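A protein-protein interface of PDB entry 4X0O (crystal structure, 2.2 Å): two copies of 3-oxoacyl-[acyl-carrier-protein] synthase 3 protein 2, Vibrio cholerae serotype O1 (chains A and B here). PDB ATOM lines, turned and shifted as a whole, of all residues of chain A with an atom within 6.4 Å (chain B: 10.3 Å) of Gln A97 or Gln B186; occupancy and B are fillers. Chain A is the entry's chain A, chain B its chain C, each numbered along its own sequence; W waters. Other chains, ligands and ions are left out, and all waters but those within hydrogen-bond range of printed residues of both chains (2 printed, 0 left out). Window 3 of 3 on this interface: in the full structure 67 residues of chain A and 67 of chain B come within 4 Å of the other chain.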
ATOM      1  N   ALA A  92      -7.246  17.804 -21.783  1.00  0.00           N
ATOM      2  CA  ALA A  92      -6.203  18.716 -22.285  1.00  0.00           C
ATOM      3  C   ALA A  92      -4.937  18.571 -21.439  1.00  0.00           C
ATOM      4  O   ALA A  92      -3.831  18.597 -21.973  1.00  0.00           O
ATOM      5  CB  ALA A  92      -6.677  20.149 -22.281  1.00  0.00           C
ATOM      6  N   SER A  93      -5.100  18.370 -20.131  1.00  0.00           N
ATOM      7  CA  SER A  93      -3.940  18.131 -19.236  1.00  0.00           C
ATOM      8  C   SER A  93      -3.234  16.766 -19.446  1.00  0.00           C
ATOM      9  O   SER A  93      -2.012  16.648 -19.264  1.00  0.00           O
ATOM     10  CB  SER A  93      -4.347  18.285 -17.775  1.00  0.00           C
ATOM     11  OG  SER A  93      -5.329  17.318 -17.394  1.00  0.00           O
ATOM     12  N   ARG A  94      -3.995  15.759 -19.851  1.00  0.00           N
ATOM     13  CA  ARG A  94      -3.426  14.477 -20.220  1.00  0.00           C
ATOM     14  C   ARG A  94      -2.590  14.619 -21.480  1.00  0.00           C
ATOM     15  O   ARG A  94      -1.481  14.112 -21.554  1.00  0.00           O
ATOM     16  CB  ARG A  94      -4.539  13.437 -20.422  1.00  0.00           C
ATOM     17  CG  ARG A  94      -4.057  12.086 -20.918  1.00  0.00           C
ATOM     18  CD  ARG A  94      -3.023  11.447 -19.994  1.00  0.00           C
ATOM     19  NE  ARG A  94      -2.659  10.119 -20.466  1.00  0.00           N
ATOM     20  CZ  ARG A  94      -1.758   9.321 -19.893  1.00  0.00           C
ATOM     21  NH1 ARG A  94      -1.099   9.702 -18.803  1.00  0.00           N
ATOM     22  NH2 ARG A  94      -1.491   8.143 -20.448  1.00  0.00           N
ATOM     23  N   VAL A  95      -3.126  15.302 -22.494  1.00  0.00           N
ATOM     24  CA  VAL A  95      -2.352  15.588 -23.719  1.00  0.00           C
ATOM     25  C   VAL A  95      -1.068  16.356 -23.363  1.00  0.00           C
ATOM     26  O   VAL A  95       0.026  16.023 -23.825  1.00  0.00           O
ATOM     27  CB  VAL A  95      -3.197  16.375 -24.754  1.00  0.00           C
ATOM     28  CG1 VAL A  95      -2.374  16.789 -25.971  1.00  0.00           C
ATOM     29  CG2 VAL A  95      -4.377  15.537 -25.219  1.00  0.00           C
ATOM     30  N   GLN A  96      -1.201  17.354 -22.500  1.00  0.00           N
ATOM     31  CA  GLN A  96      -0.065  18.121 -22.015  1.00  0.00           C
ATOM     32  C   GLN A  96       0.974  17.254 -21.333  1.00  0.00           C
ATOM     33  O   GLN A  96       2.185  17.370 -21.596  1.00  0.00           O
ATOM     34  CB  GLN A  96      -0.548  19.180 -21.039  1.00  0.00           C
ATOM     35  CG  GLN A  96       0.486  20.250 -20.763  1.00  0.00           C
ATOM     36  CD  GLN A  96       0.049  21.208 -19.670  1.00  0.00           C
ATOM     37  OE1 GLN A  96      -1.117  21.281 -19.333  1.00  0.00           O
ATOM     38  NE2 GLN A  96       0.982  21.973 -19.153  1.00  0.00           N
ATOM     39  N   GLN A  97       0.503  16.366 -20.463  1.00  0.00           N
ATOM     40  CA  GLN A  97       1.369  15.436 -19.768  1.00  0.00           C
ATOM     41  C   GLN A  97       2.072  14.501 -20.763  1.00  0.00           C
ATOM     42  O   GLN A  97       3.258  14.252 -20.647  1.00  0.00           O
ATOM     43  CB  GLN A  97       0.547  14.628 -18.734  1.00  0.00           C
ATOM     44  CG  GLN A  97       1.377  13.769 -17.784  1.00  0.00           C
ATOM     45  CD  GLN A  97       0.533  12.774 -16.992  1.00  0.00           C
ATOM     46  OE1 GLN A  97      -0.440  12.223 -17.501  1.00  0.00           O
ATOM     47  NE2 GLN A  97       0.898  12.553 -15.745  1.00  0.00           N
ATOM     48  N   ASN A  98       1.335  13.957 -21.719  1.00  0.00           N
ATOM     49  CA  ASN A  98       1.929  13.048 -22.714  1.00  0.00           C
ATOM     50  C   ASN A  98       3.016  13.720 -23.552  1.00  0.00           C
ATOM     51  O   ASN A  98       4.008  13.104 -23.870  1.00  0.00           O
ATOM     52  CB  ASN A  98       0.869  12.498 -23.663  1.00  0.00           C
ATOM     53  CG  ASN A  98      -0.119  11.573 -22.993  1.00  0.00           C
ATOM     54  OD1 ASN A  98       0.138  11.030 -21.920  1.00  0.00           O
ATOM     55  ND2 ASN A  98      -1.260  11.373 -23.638  1.00  0.00           N
ATOM     56  N   LEU A  99       2.817  14.985 -23.909  1.00  0.00           N
ATOM     57  CA  LEU A  99       3.767  15.693 -24.748  1.00  0.00           C
ATOM     58  C   LEU A  99       4.891  16.363 -23.989  1.00  0.00           C
ATOM     59  O   LEU A  99       5.842  16.811 -24.605  1.00  0.00           O
ATOM     60  CB  LEU A  99       3.067  16.741 -25.597  1.00  0.00           C
ATOM     61  CG  LEU A  99       1.914  16.272 -26.487  1.00  0.00           C
ATOM     62  CD1 LEU A  99       1.396  17.449 -27.290  1.00  0.00           C
ATOM     63  CD2 LEU A  99       2.330  15.176 -27.444  1.00  0.00           C
ATOM     64  N   GLY A 100       4.795  16.441 -22.664  1.00  0.00           N
ATOM     65  CA  GLY A 100       5.813  17.143 -21.888  1.00  0.00           C
ATOM     66  C   GLY A 100       5.802  18.651 -22.122  1.00  0.00           C
ATOM     67  O   GLY A 100       6.846  19.297 -22.040  1.00  0.00           O
ATOM     68  N   ILE A 101       4.629  19.228 -22.385  1.00  0.00           N
ATOM     69  CA  ILE A 101       4.511  20.684 -22.475  1.00  0.00           C
ATOM     70  C   ILE A 101       4.443  21.266 -21.052  1.00  0.00           C
ATOM     71  O   ILE A 101       3.538  20.927 -20.303  1.00  0.00           O
ATOM     72  CB  ILE A 101       3.261  21.096 -23.281  1.00  0.00           C
ATOM     73  CG1 ILE A 101       3.394  20.610 -24.726  1.00  0.00           C
ATOM     74  CG2 ILE A 101       3.052  22.612 -23.259  1.00  0.00           C
ATOM     75  CD1 ILE A 101       2.113  20.656 -25.501  1.00  0.00           C
ATOM     76  N   GLY B 182      -2.593  28.501 -16.177  1.00  0.00           N
ATOM     77  CA  GLY B 182      -1.728  27.475 -16.652  1.00  0.00           C
ATOM     78  C   GLY B 182      -2.079  26.125 -16.096  1.00  0.00           C
ATOM     79  O   GLY B 182      -3.132  25.939 -15.516  1.00  0.00           O
ATOM     80  N   CYS B 183      -1.172  25.177 -16.277  1.00  0.00           N
ATOM     81  CA  CYS B 183      -1.383  23.816 -15.824  1.00  0.00           C
ATOM     82  C   CYS B 183      -0.037  23.144 -15.697  1.00  0.00           C
ATOM     83  O   CYS B 183       0.800  23.209 -16.623  1.00  0.00           O
ATOM     84  CB  CYS B 183      -2.315  23.044 -16.799  1.00  0.00           C
ATOM     85  SG  CYS B 183      -2.735  21.351 -16.284  1.00  0.00           S
ATOM     86  N   ASP B 184       0.171  22.517 -14.543  1.00  0.00           N
ATOM     87  CA  ASP B 184       1.383  21.742 -14.257  1.00  0.00           C
ATOM     88  C   ASP B 184       0.971  20.285 -14.395  1.00  0.00           C
ATOM     89  O   ASP B 184       0.484  19.638 -13.442  1.00  0.00           O
ATOM     90  CB  ASP B 184       1.945  22.038 -12.854  1.00  0.00           C
ATOM     91  CG  ASP B 184       2.679  23.410 -12.732  1.00  0.00           C
ATOM     92  OD1 ASP B 184       2.768  24.179 -13.704  1.00  0.00           O
ATOM     93  OD2 ASP B 184       3.185  23.732 -11.624  1.00  0.00           O
ATOM     94  N   ALA B 185       1.119  19.788 -15.619  1.00  0.00           N
ATOM     95  CA  ALA B 185       0.535  18.516 -16.005  1.00  0.00           C
ATOM     96  C   ALA B 185       1.272  17.307 -15.432  1.00  0.00           C
ATOM     97  O   ALA B 185       0.712  16.210 -15.375  1.00  0.00           O
ATOM     98  CB  ALA B 185       0.442  18.431 -17.522  1.00  0.00           C
ATOM     99  N   GLN B 186       2.510  17.482 -15.000  1.00  0.00           N
ATOM    100  CA  GLN B 186       3.255  16.337 -14.503  1.00  0.00           C
ATOM    101  C   GLN B 186       2.653  15.800 -13.196  1.00  0.00           C
ATOM    102  O   GLN B 186       2.817  14.617 -12.877  1.00  0.00           O
ATOM    103  CB  GLN B 186       4.745  16.654 -14.365  1.00  0.00           C
ATOM    104  CG  GLN B 186       5.455  16.918 -15.691  1.00  0.00           C
ATOM    105  CD  GLN B 186       5.347  15.793 -16.725  1.00  0.00           C
ATOM    106  OE1 GLN B 186       5.146  16.057 -17.916  1.00  0.00           O
ATOM    107  NE2 GLN B 186       5.470  14.539 -16.280  1.00  0.00           N
ATOM    108  N   GLY B 187       1.948  16.653 -12.460  1.00  0.00           N
ATOM    109  CA  GLY B 187       1.283  16.244 -11.227  1.00  0.00           C
ATOM    110  C   GLY B 187      -0.191  15.896 -11.402  1.00  0.00           C
ATOM    111  O   GLY B 187      -0.954  15.899 -10.437  1.00  0.00           O
ATOM    112  N   ARG B 188      -0.572  15.540 -12.619  1.00  0.00           N
ATOM    113  CA  ARG B 188      -1.955  15.253 -12.974  1.00  0.00           C
ATOM    114  C   ARG B 188      -2.592  14.084 -12.191  1.00  0.00           C
ATOM    115  O   ARG B 188      -3.798  14.071 -11.948  1.00  0.00           O
ATOM    116  CB  ARG B 188      -2.013  14.960 -14.475  1.00  0.00           C
ATOM    117  CG  ARG B 188      -3.403  14.760 -15.022  1.00  0.00           C
ATOM    118  CD  ARG B 188      -3.396  14.519 -16.511  1.00  0.00           C
ATOM    119  NE  ARG B 188      -4.772  14.438 -16.982  1.00  0.00           N
ATOM    120  CZ  ARG B 188      -5.497  13.326 -17.029  1.00  0.00           C
ATOM    121  NH1 ARG B 188      -4.978  12.161 -16.640  1.00  0.00           N
ATOM    122  NH2 ARG B 188      -6.753  13.369 -17.482  1.00  0.00           N
ATOM    123  N   ASP B 189      -1.785  13.110 -11.796  1.00  0.00           N
ATOM    124  CA  ASP B 189      -2.321  11.873 -11.219  1.00  0.00           C
ATOM    125  C   ASP B 189      -2.690  11.961  -9.733  1.00  0.00           C
ATOM    126  O   ASP B 189      -3.348  11.061  -9.212  1.00  0.00           O
ATOM    127  CB  ASP B 189      -1.337  10.731 -11.472  1.00  0.00           C
ATOM    128  CG  ASP B 189      -1.100  10.496 -12.964  1.00  0.00           C
ATOM    129  OD1 ASP B 189      -2.085  10.325 -13.714  1.00  0.00           O
ATOM    130  OD2 ASP B 189       0.068  10.501 -13.402  1.00  0.00           O
ATOM    131  N   ILE B 190      -2.310  13.051  -9.065  1.00  0.00           N
ATOM    132  CA  ILE B 190      -2.523  13.171  -7.617  1.00  0.00           C
ATOM    133  C   ILE B 190      -3.915  13.693  -7.239  1.00  0.00           C
ATOM    134  O   ILE B 190      -4.251  13.739  -6.058  1.00  0.00           O
ATOM    135  CB  ILE B 190      -1.436  14.040  -6.935  1.00  0.00           C
ATOM    136  CG1 ILE B 190      -1.680  15.539  -7.179  1.00  0.00           C
ATOM    137  CG2 ILE B 190      -0.041  13.585  -7.367  1.00  0.00           C
ATOM    138  CD1 ILE B 190      -0.523  16.425  -6.753  1.00  0.00           C
ATOM    139  N   LEU B 191      -4.722  14.061  -8.230  1.00  0.00           N
ATOM    140  CA  LEU B 191      -6.085  14.557  -7.996  1.00  0.00           C
ATOM    141  C   LEU B 191      -6.961  14.252  -9.200  1.00  0.00           C
ATOM    142  O   LEU B 191      -6.951  14.988 -10.208  1.00  0.00           O
ATOM    143  CB  LEU B 191      -6.036  16.052  -7.724  1.00  0.00           C
ATOM    144  CG  LEU B 191      -7.338  16.812  -7.501  1.00  0.00           C
ATOM    145  CD1 LEU B 191      -8.322  16.038  -6.646  1.00  0.00           C
ATOM    146  CD2 LEU B 191      -7.039  18.175  -6.884  1.00  0.00           C
ATOM    147  N   ALA B 192      -7.678  13.132  -9.111  1.00  0.00           N
ATOM    148  CA  ALA B 192      -8.269  12.492 -10.284  1.00  0.00           C
ATOM    149  C   ALA B 192      -9.366  11.484  -9.941  1.00  0.00           C
ATOM    150  O   ALA B 192      -9.282  10.774  -8.941  1.00  0.00           O
ATOM    151  CB  ALA B 192      -7.181  11.784 -11.073  1.00  0.00           C
ATOM    152  N   PRO B 194     -10.256   8.862 -12.402  1.00  0.00           N
ATOM    153  CA  PRO B 194      -9.954   8.423 -13.776  1.00  0.00           C
ATOM    154  C   PRO B 194     -11.061   7.625 -14.473  1.00  0.00           C
ATOM    155  O   PRO B 194     -11.053   7.528 -15.707  1.00  0.00           O
ATOM    156  CB  PRO B 194      -8.708   7.542 -13.600  1.00  0.00           C
ATOM    157  CG  PRO B 194      -8.156   7.892 -12.261  1.00  0.00           C
ATOM    158  CD  PRO B 194      -9.332   8.273 -11.426  1.00  0.00           C
ATOM    159  N   GLU B 218       0.713  16.582  -1.269  1.00  0.00           N
ATOM    160  CA  GLU B 218       1.335  17.059  -2.506  1.00  0.00           C
ATOM    161  C   GLU B 218       0.478  18.137  -3.159  1.00  0.00           C
ATOM    162  O   GLU B 218       1.007  19.112  -3.682  1.00  0.00           O
ATOM    163  CB  GLU B 218       1.583  15.905  -3.495  1.00  0.00           C
ATOM    164  CG  GLU B 218       2.897  15.163  -3.288  1.00  0.00           C
ATOM    165  CD  GLU B 218       4.121  16.021  -3.576  1.00  0.00           C
ATOM    166  OE1 GLU B 218       4.028  16.948  -4.419  1.00  0.00           O
ATOM    167  OE2 GLU B 218       5.188  15.755  -2.961  1.00  0.00           O
ATOM    168  N   ARG B 222       1.906  21.912  -3.978  1.00  0.00           N
ATOM    169  CA  ARG B 222       1.859  22.411  -5.342  1.00  0.00           C
ATOM    170  C   ARG B 222       0.874  23.577  -5.556  1.00  0.00           C
ATOM    171  O   ARG B 222       1.106  24.440  -6.400  1.00  0.00           O
ATOM    172  CB  ARG B 222       1.514  21.271  -6.310  1.00  0.00           C
ATOM    173  CG  ARG B 222       2.592  20.205  -6.440  1.00  0.00           C
ATOM    174  CD  ARG B 222       2.057  19.081  -7.302  1.00  0.00           C
ATOM    175  NE  ARG B 222       3.024  18.054  -7.652  1.00  0.00           N
ATOM    176  CZ  ARG B 222       3.864  18.151  -8.674  1.00  0.00           C
ATOM    177  NH1 ARG B 222       4.691  17.151  -8.941  1.00  0.00           N
ATOM    178  NH2 ARG B 222       3.892  19.251  -9.414  1.00  0.00           N
ATOM    179  N   GLY B 312      -6.459  23.556  -9.183  1.00  0.00           N
ATOM    180  CA  GLY B 312      -7.325  22.397  -9.348  1.00  0.00           C
ATOM    181  C   GLY B 312      -6.698  21.214 -10.020  1.00  0.00           C
ATOM    182  O   GLY B 312      -5.514  21.235 -10.384  1.00  0.00           O
ATOM    183  N   ALA B 313      -7.510  20.171 -10.191  1.00  0.00           N
ATOM    184  CA  ALA B 313      -7.071  18.970 -10.905  1.00  0.00           C
ATOM    185  C   ALA B 313      -6.445  19.373 -12.236  1.00  0.00           C
ATOM    186  O   ALA B 313      -6.930  20.287 -12.905  1.00  0.00           O
ATOM    187  CB  ALA B 313      -8.252  18.040 -11.140  1.00  0.00           C
ATOM    188  N   GLY B 314      -5.368  18.703 -12.632  1.00  0.00           N
ATOM    189  CA  GLY B 314      -4.721  19.038 -13.891  1.00  0.00           C
ATOM    190  C   GLY B 314      -3.235  18.870 -13.946  1.00  0.00           C
ATOM    191  O   GLY B 314      -2.744  18.217 -14.839  1.00  0.00           O
ATOM    192  N   LEU B 315      -2.480  19.485 -13.047  1.00  0.00           N
ATOM    193  CA  LEU B 315      -2.962  20.450 -12.072  1.00  0.00           C
ATOM    194  C   LEU B 315      -3.084  21.864 -12.644  1.00  0.00           C
ATOM    195  O   LEU B 315      -2.084  22.534 -12.886  1.00  0.00           O
ATOM    196  CB  LEU B 315      -1.996  20.467 -10.933  1.00  0.00           C
ATOM    197  N   THR B 316      -4.315  22.320 -12.814  1.00  0.00           N
ATOM    198  CA  THR B 316      -4.565  23.646 -13.352  1.00  0.00           C
ATOM    199  C   THR B 316      -4.348  24.709 -12.286  1.00  0.00           C
ATOM    200  O   THR B 316      -4.423  24.429 -11.079  1.00  0.00           O
ATOM    201  CB  THR B 316      -5.986  23.791 -13.883  1.00  0.00           C
ATOM    202  OG1 THR B 316      -6.930  23.458 -12.858  1.00  0.00           O
ATOM    203  CG2 THR B 316      -6.185  22.908 -15.091  1.00  0.00           C
ATOM    204  N   TRP B 317      -3.996  25.904 -12.750  1.00  0.00           N
ATOM    205  CA  TRP B 317      -3.712  26.976 -11.838  1.00  0.00           C
ATOM    206  C   TRP B 317      -3.936  28.320 -12.521  1.00  0.00           C
ATOM    207  O   TRP B 317      -3.968  28.434 -13.775  1.00  0.00           O
ATOM    208  CB  TRP B 317      -2.294  26.897 -11.243  1.00  0.00           C
ATOM    209  CG  TRP B 317      -1.131  26.775 -12.227  1.00  0.00           C
ATOM    210  CD1 TRP B 317      -0.448  25.645 -12.523  1.00  0.00           C
ATOM    211  CD2 TRP B 317      -0.524  27.822 -13.010  1.00  0.00           C
ATOM    212  NE1 TRP B 317       0.548  25.908 -13.435  1.00  0.00           N
ATOM    213  CE2 TRP B 317       0.512  27.239 -13.756  1.00  0.00           C
ATOM    214  CE3 TRP B 317      -0.764  29.189 -13.152  1.00  0.00           C
ATOM    215  CZ2 TRP B 317       1.321  27.981 -14.641  1.00  0.00           C
ATOM    216  CZ3 TRP B 317       0.044  29.932 -14.028  1.00  0.00           C
ATOM    217  CH2 TRP B 317       1.042  29.321 -14.772  1.00  0.00           C
HETATM  218  O   HOH W   1       3.959  18.473 -18.705  1.00  0.00           O
HETATM  219  O   HOH W   2       1.163  12.633 -12.618  1.00  0.00           O
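Ser A93 touches Cys B183 (CB to SG, 3.8 Å).
O of Ser A93 touches CB of Ala B185, at 3.5 Å.
O of Gly B314 touches CB of Ser A93, at 3.3 Å.
Gln A96 touches Ala B185 (CD to CB, 3.5 Å).
O of Ala B185 touches CG of Gln A97 (3.5 Å).
OE1 of Gln B186 touches O of Gln A97 (3.8 Å).
Arg B188 touches Gln A97 (CD to OE1, 3.9 Å).
Water W2 lies within hydrogen-bond range of the side-chain carboxylate (OD2) of Asp B189, the backbone carbonyl oxygen (O) of Gln B186, the side-chain amide nitrogen (NE2) of Gln A97 and the backbone NH (N) of Arg B188.
Water W1 bridges the side-chain amide oxygen (OE1) of Gln B186 (2.8 Å) and the backbone carbonyl oxygen (O) of Ile A101 (3.0 Å).
No position is printed for both chains.
Of the 10 printed residues of chain A, 4 touch a printed residue of chain B.
Along chain A the printed residues that touch a printed residue of chain B span positions 93 to 97.
Of the 20 printed residues of chain B, 6 touch a printed residue of chain A.
Printed residues of chain B that touch a printed residue of chain A: Cys B183, Ala B185, Gln B186, Arg B188, Asp B189 and Gly B314.
Hydrophobic or aromatic side chains of chain B within 4 Å of the printed part of chain A: Ala B185.
Among the printed residues, 11 pairs touch across the chains.
Among the printed residues, no Asp or Glu carboxylate lies within 4 Å of a Lys or Arg side-chain nitrogen of the other chain.
The side-chain sulfur (SG) of Cys B183 lies close to the backbone carbonyl oxygen (O) of Leu B315 (3.7 Å).
The side-chain sulfur of Cys B183 lies close to the backbone carbonyl oxygen of Gly B314 (3.5 Å).
The guanidinium group of Arg A94 lies within hydrogen-bond range of the side-chain amide oxygen of Gln A97.
NE of Arg A94 sits close to OD1 of Asn A98 (3.3 Å).
The side-chain amide nitrogen (NE2) of Gln A96 sits at hydrogen-bond distance from the backbone carbonyl oxygen (O) of Ile A101.
NE of Arg B188 sits close to N of Arg A94 (3.3 Å).
OD2 of Asp B189 is in hydrogen-bond range of NE2 of Gln A97.
The backbone carbonyl oxygen (O) of Cys B183 sits at hydrogen-bond distance from the side-chain amide nitrogen (NE2) of Gln A96 (2.8 Å).
The guanidinium group (NE) of Arg B188 lies within hydrogen-bond range of the side-chain hydroxyl (OG) of Ser A93.
Gln A97 touches four residues of chain B.
Arg A94 touches just one residue of chain B: Arg B188 (3.3 Å).
Of chain B, only Cys B183 (2.8 Å) and Ala B185 (3.5 Å) come within 4 Å of Gln A96.
No residue of chain B comes within 4 Å of Gly A100.
Of the printed residues of chain A, Cys B183 touches Ser A93 (3.8 Å) and Gln A96 (2.8 Å).
Printed residues of chain A within 4 Å of Ala B185: Ser A93 (3.5 Å), Gln A96 (3.5 Å) and Gln A97 (3.5 Å).
Of the printed residues of chain A, Gly B314 touches Ser A93 (3.3 Å).
Of the printed residues of chain B, Ser A93 touches Cys B183 (3.8 Å), Ala B185 (3.5 Å), Arg B188 (3.0 Å) and Gly B314 (3.3 Å).
Ala B313 touches none of the printed residues of chain A.
Thr B316 touches none of the printed residues of chain A.
The nearest residue of chain B that does not touch Gln A97 is Gly B187 (5.4 Å).
The nearest printed residue of chain A that does not touch Ala B185 is Ile A101 (4.9 Å).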
